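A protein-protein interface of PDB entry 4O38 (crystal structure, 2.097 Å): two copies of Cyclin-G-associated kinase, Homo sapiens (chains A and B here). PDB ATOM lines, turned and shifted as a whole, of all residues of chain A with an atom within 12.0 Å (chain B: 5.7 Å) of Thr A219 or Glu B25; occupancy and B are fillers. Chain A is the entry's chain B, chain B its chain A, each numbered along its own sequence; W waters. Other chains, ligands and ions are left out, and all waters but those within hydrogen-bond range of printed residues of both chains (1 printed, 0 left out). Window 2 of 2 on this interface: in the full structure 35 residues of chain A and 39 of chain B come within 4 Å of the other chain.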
ATOM      1  N   THR A 219      23.134 -31.652   6.248  1.00  0.00           N
ATOM      2  CA  THR A 219      22.960 -30.655   5.186  1.00  0.00           C
ATOM      3  C   THR A 219      21.625 -30.885   4.442  1.00  0.00           C
ATOM      4  O   THR A 219      21.190 -32.052   4.252  1.00  0.00           O
ATOM      5  CB  THR A 219      24.130 -30.683   4.150  1.00  0.00           C
ATOM      6  OG1 THR A 219      23.978 -31.808   3.262  1.00  0.00           O
ATOM      7  CG2 THR A 219      25.516 -30.740   4.851  1.00  0.00           C
ATOM      8  N   PRO A 220      20.983 -29.783   4.004  1.00  0.00           N
ATOM      9  CA  PRO A 220      19.708 -29.898   3.284  1.00  0.00           C
ATOM     10  C   PRO A 220      19.806 -30.589   1.925  1.00  0.00           C
ATOM     11  O   PRO A 220      20.843 -30.575   1.278  1.00  0.00           O
ATOM     12  CB  PRO A 220      19.238 -28.433   3.117  1.00  0.00           C
ATOM     13  CG  PRO A 220      20.354 -27.565   3.565  1.00  0.00           C
ATOM     14  CD  PRO A 220      21.334 -28.380   4.329  1.00  0.00           C
ATOM     15  N   GLU A 221      18.701 -31.185   1.510  1.00  0.00           N
ATOM     16  CA  GLU A 221      18.632 -31.890   0.247  1.00  0.00           C
ATOM     17  C   GLU A 221      18.060 -30.947  -0.823  1.00  0.00           C
ATOM     18  O   GLU A 221      16.965 -30.444  -0.669  1.00  0.00           O
ATOM     19  CB  GLU A 221      17.761 -33.137   0.420  1.00  0.00           C
ATOM     20  CG  GLU A 221      18.247 -34.016   1.570  1.00  0.00           C
ATOM     21  CD  GLU A 221      17.117 -34.656   2.375  1.00  0.00           C
ATOM     22  OE1 GLU A 221      16.898 -34.241   3.548  1.00  0.00           O
ATOM     23  OE2 GLU A 221      16.452 -35.576   1.831  1.00  0.00           O
ATOM     24  N   ILE A 222      18.831 -30.691  -1.886  1.00  0.00           N
ATOM     25  CA  ILE A 222      18.346 -29.905  -3.024  1.00  0.00           C
ATOM     26  C   ILE A 222      17.054 -30.565  -3.538  1.00  0.00           C
ATOM     27  O   ILE A 222      16.971 -31.787  -3.592  1.00  0.00           O
ATOM     28  CB  ILE A 222      19.402 -29.766  -4.148  1.00  0.00           C
ATOM     29  CG1 ILE A 222      20.628 -28.984  -3.625  1.00  0.00           C
ATOM     30  CG2 ILE A 222      18.774 -29.104  -5.387  1.00  0.00           C
ATOM     31  CD1 ILE A 222      21.513 -28.366  -4.701  1.00  0.00           C
ATOM     32  N   ILE A 223      16.046 -29.746  -3.865  1.00  0.00           N
ATOM     33  CA  ILE A 223      14.716 -30.236  -4.257  1.00  0.00           C
ATOM     34  C   ILE A 223      14.788 -30.836  -5.675  1.00  0.00           C
ATOM     35  O   ILE A 223      15.200 -30.147  -6.628  1.00  0.00           O
ATOM     36  CB  ILE A 223      13.647 -29.102  -4.150  1.00  0.00           C
ATOM     37  CG1 ILE A 223      13.111 -29.008  -2.705  1.00  0.00           C
ATOM     38  CG2 ILE A 223      12.494 -29.300  -5.141  1.00  0.00           C
ATOM     39  CD1 ILE A 223      12.315 -27.754  -2.419  1.00  0.00           C
ATOM     40  N   PHE A 229       7.464 -35.379   0.177  1.00  0.00           N
ATOM     41  CA  PHE A 229       6.676 -34.702   1.156  1.00  0.00           C
ATOM     42  C   PHE A 229       5.269 -35.031   0.795  1.00  0.00           C
ATOM     43  O   PHE A 229       4.911 -34.997  -0.380  1.00  0.00           O
ATOM     44  CB  PHE A 229       6.928 -33.188   1.077  1.00  0.00           C
ATOM     45  CG  PHE A 229       8.280 -32.813   1.644  1.00  0.00           C
ATOM     46  CD1 PHE A 229       8.477 -32.805   3.045  1.00  0.00           C
ATOM     47  CD2 PHE A 229       9.363 -32.615   0.818  1.00  0.00           C
ATOM     48  CE1 PHE A 229       9.721 -32.527   3.604  1.00  0.00           C
ATOM     49  CE2 PHE A 229      10.615 -32.337   1.364  1.00  0.00           C
ATOM     50  CZ  PHE A 229      10.797 -32.312   2.759  1.00  0.00           C
ATOM     51  N   THR B  23      25.619 -21.556   9.163  1.00  0.00           N
ATOM     52  CA  THR B  23      26.071 -21.724   7.818  1.00  0.00           C
ATOM     53  C   THR B  23      25.238 -22.835   7.228  1.00  0.00           C
ATOM     54  O   THR B  23      25.004 -23.830   7.870  1.00  0.00           O
ATOM     55  CB  THR B  23      27.563 -22.065   7.767  1.00  0.00           C
ATOM     56  OG1 THR B  23      28.329 -20.916   8.176  1.00  0.00           O
ATOM     57  CG2 THR B  23      27.971 -22.405   6.377  1.00  0.00           C
ATOM     58  N   VAL B  24      24.780 -22.669   6.000  1.00  0.00           N
ATOM     59  CA  VAL B  24      23.836 -23.626   5.412  1.00  0.00           C
ATOM     60  C   VAL B  24      24.451 -24.078   4.100  1.00  0.00           C
ATOM     61  O   VAL B  24      24.823 -23.258   3.255  1.00  0.00           O
ATOM     62  CB  VAL B  24      22.470 -22.922   5.186  1.00  0.00           C
ATOM     63  CG1 VAL B  24      21.582 -23.702   4.263  1.00  0.00           C
ATOM     64  CG2 VAL B  24      21.764 -22.769   6.518  1.00  0.00           C
ATOM     65  N   GLU B  25      24.528 -25.362   3.892  1.00  0.00           N
ATOM     66  CA  GLU B  25      25.048 -25.882   2.652  1.00  0.00           C
ATOM     67  C   GLU B  25      23.912 -26.184   1.646  1.00  0.00           C
ATOM     68  O   GLU B  25      22.983 -26.894   1.966  1.00  0.00           O
ATOM     69  CB  GLU B  25      25.808 -27.131   2.922  1.00  0.00           C
ATOM     70  CG  GLU B  25      27.203 -26.869   3.415  1.00  0.00           C
ATOM     71  CD  GLU B  25      28.149 -27.999   3.013  1.00  0.00           C
ATOM     72  OE1 GLU B  25      29.291 -27.649   2.684  1.00  0.00           O
ATOM     73  OE2 GLU B  25      27.746 -29.213   2.996  1.00  0.00           O
ATOM     74  N   LEU B  26      24.021 -25.675   0.449  1.00  0.00           N
ATOM     75  CA  LEU B  26      23.090 -25.931  -0.669  1.00  0.00           C
ATOM     76  C   LEU B  26      23.948 -26.252  -1.898  1.00  0.00           C
ATOM     77  O   LEU B  26      24.513 -25.340  -2.524  1.00  0.00           O
ATOM     78  CB  LEU B  26      22.245 -24.655  -0.957  1.00  0.00           C
ATOM     79  CG  LEU B  26      20.796 -24.601  -0.499  1.00  0.00           C
ATOM     80  CD1 LEU B  26      20.758 -24.958   0.962  1.00  0.00           C
ATOM     81  CD2 LEU B  26      20.123 -23.239  -0.659  1.00  0.00           C
ATOM     82  N   GLY B  27      24.085 -27.508  -2.203  1.00  0.00           N
ATOM     83  CA  GLY B  27      24.993 -27.998  -3.243  1.00  0.00           C
ATOM     84  C   GLY B  27      26.393 -27.495  -2.960  1.00  0.00           C
ATOM     85  O   GLY B  27      26.923 -27.709  -1.873  1.00  0.00           O
ATOM     86  N   LEU B  29      27.173 -24.382  -2.661  1.00  0.00           N
ATOM     87  CA  LEU B  29      27.145 -23.164  -1.858  1.00  0.00           C
ATOM     88  C   LEU B  29      27.269 -23.467  -0.372  1.00  0.00           C
ATOM     89  O   LEU B  29      26.731 -24.478   0.145  1.00  0.00           O
ATOM     90  CB  LEU B  29      25.917 -22.349  -2.143  1.00  0.00           C
ATOM     91  CG  LEU B  29      25.648 -22.116  -3.618  1.00  0.00           C
ATOM     92  CD1 LEU B  29      24.297 -21.431  -3.812  1.00  0.00           C
ATOM     93  CD2 LEU B  29      26.745 -21.272  -4.265  1.00  0.00           C
ATOM     94  N   ARG B  30      28.030 -22.633   0.296  1.00  0.00           N
ATOM     95  CA  ARG B  30      28.155 -22.611   1.756  1.00  0.00           C
ATOM     96  C   ARG B  30      27.777 -21.224   2.221  1.00  0.00           C
ATOM     97  O   ARG B  30      28.547 -20.285   2.116  1.00  0.00           O
ATOM     98  CB  ARG B  30      29.559 -22.980   2.141  1.00  0.00           C
ATOM     99  CG  ARG B  30      29.847 -22.995   3.628  1.00  0.00           C
ATOM    100  CD  ARG B  30      31.177 -23.712   3.871  1.00  0.00           C
ATOM    101  NE  ARG B  30      31.030 -25.174   3.753  1.00  0.00           N
ATOM    102  CZ  ARG B  30      32.011 -26.076   3.544  1.00  0.00           C
ATOM    103  NH1 ARG B  30      33.287 -25.737   3.365  1.00  0.00           N
ATOM    104  NH2 ARG B  30      31.682 -27.370   3.515  1.00  0.00           N
ATOM    105  N   LEU B  31      26.547 -21.102   2.680  1.00  0.00           N
ATOM    106  CA  LEU B  31      25.926 -19.823   2.863  1.00  0.00           C
ATOM    107  C   LEU B  31      25.938 -19.382   4.339  1.00  0.00           C
ATOM    108  O   LEU B  31      25.287 -20.015   5.175  1.00  0.00           O
ATOM    109  CB  LEU B  31      24.487 -19.892   2.387  1.00  0.00           C
ATOM    110  CG  LEU B  31      24.370 -20.226   0.871  1.00  0.00           C
ATOM    111  CD1 LEU B  31      23.001 -20.756   0.637  1.00  0.00           C
ATOM    112  CD2 LEU B  31      24.649 -18.985   0.049  1.00  0.00           C
ATOM    113  N   SER B  97      15.320 -28.800   0.927  1.00  0.00           N
ATOM    114  CA  SER B  97      14.452 -29.190   2.036  1.00  0.00           C
ATOM    115  C   SER B  97      15.200 -29.979   3.079  1.00  0.00           C
ATOM    116  O   SER B  97      16.110 -30.736   2.758  1.00  0.00           O
ATOM    117  CB  SER B  97      13.324 -30.066   1.540  1.00  0.00           C
ATOM    118  OG  SER B  97      13.819 -31.144   0.784  1.00  0.00           O
ATOM    119  N   ILE B  98      14.806 -29.791   4.326  1.00  0.00           N
ATOM    120  CA  ILE B  98      15.238 -30.616   5.438  1.00  0.00           C
ATOM    121  C   ILE B  98      13.976 -31.321   5.992  1.00  0.00           C
ATOM    122  O   ILE B  98      12.989 -30.667   6.347  1.00  0.00           O
ATOM    123  CB  ILE B  98      15.881 -29.750   6.522  1.00  0.00           C
ATOM    124  CG1 ILE B  98      16.983 -28.898   5.894  1.00  0.00           C
ATOM    125  CG2 ILE B  98      16.442 -30.609   7.642  1.00  0.00           C
ATOM    126  CD1 ILE B  98      17.703 -27.958   6.840  1.00  0.00           C
ATOM    127  N   GLU B 102      15.251 -34.681  10.695  1.00  0.00           N
ATOM    128  CA  GLU B 102      16.638 -34.202  10.578  1.00  0.00           C
ATOM    129  C   GLU B 102      16.758 -32.679  10.758  1.00  0.00           C
ATOM    130  O   GLU B 102      17.857 -32.153  10.771  1.00  0.00           O
ATOM    131  CB  GLU B 102      17.333 -34.717   9.302  1.00  0.00           C
ATOM    132  CG  GLU B 102      16.697 -34.337   7.980  1.00  0.00           C
ATOM    133  CD  GLU B 102      16.852 -35.420   6.925  1.00  0.00           C
ATOM    134  OE1 GLU B 102      17.526 -35.167   5.906  1.00  0.00           O
ATOM    135  OE2 GLU B 102      16.311 -36.527   7.114  1.00  0.00           O
HETATM  136  O   HOH W   1      23.040 -29.626  -0.478  1.00  0.00           O
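O of Glu A221 is in hydrogen-bond range of N of Ser B97, 2.8 Å away.
The side-chain carboxylate (OE1) of Glu B102 lies close to the side-chain carboxylate (OE1) of Glu A221 (2.6 Å).
NH2 of Arg B30 is in salt-bridge range of OE1 of Glu B25 (2.5 Å).
Among the printed residues, pairs that only touch across the chains: Thr A219 with Glu B25 (3.3 Å), Pro A220 with Glu B25 (3.1 Å), Pro A220 with Leu B26 (3.7 Å), Pro A220 with Ser B97 (3.7 Å), Pro A220 with Ile B98 (3.6 Å), Ile A222 with Gly B27 (3.7 Å) and Phe A229 with Ser B97 (3.5 Å).
Printed residues of chain B within 4 Å of Glu A221: Ser B97 (2.8 Å) and Glu B102 (2.6 Å).
Printed residues of chain B within 4 Å of Ile A222: Gly B27.
Ile A223 touches none of the printed residues of chain B.
No residue of chain A comes within 4 Å of Val B24.
Glu B25 touches two residues of chain A.
Gly B27 touches just one residue of chain A: Ile A222.
No residue of chain A comes within 4 Å of Arg B30.
No residue of chain A comes within 4 Å of Leu B31.
Of the printed residues of chain A, Ser B97 touches Pro A220 (3.7 Å), Glu A221 (2.8 Å) and Phe A229 (3.5 Å).
Printed residues of chain A within 4 Å of Glu B102: Glu A221.
The nearest residue of chain A that does not touch Glu B25 is Glu A221 (6.1 Å).
The nearest printed residue of chain B that does not touch Phe A229 is Ile B98 (4.5 Å).
Of the 11 printed residues of chain B, 6 touch a printed residue of chain A.
Hydrophobic or aromatic side chains of chain B within 4 Å of the printed part of chain A: Leu B26 and Ile B98.
Among the printed residues, 9 pairs touch across the chains.
Among the printed residues, no Asp or Glu carboxylate lies within 4 Å of a Lys or Arg side-chain nitrogen of the other chain.
No position is printed for both chains.
Water W1 bridges the backbone NH (N) of Gly B27 (2.9 Å) and the backbone carbonyl oxygen (O) of Pro A220 (3.0 Å).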
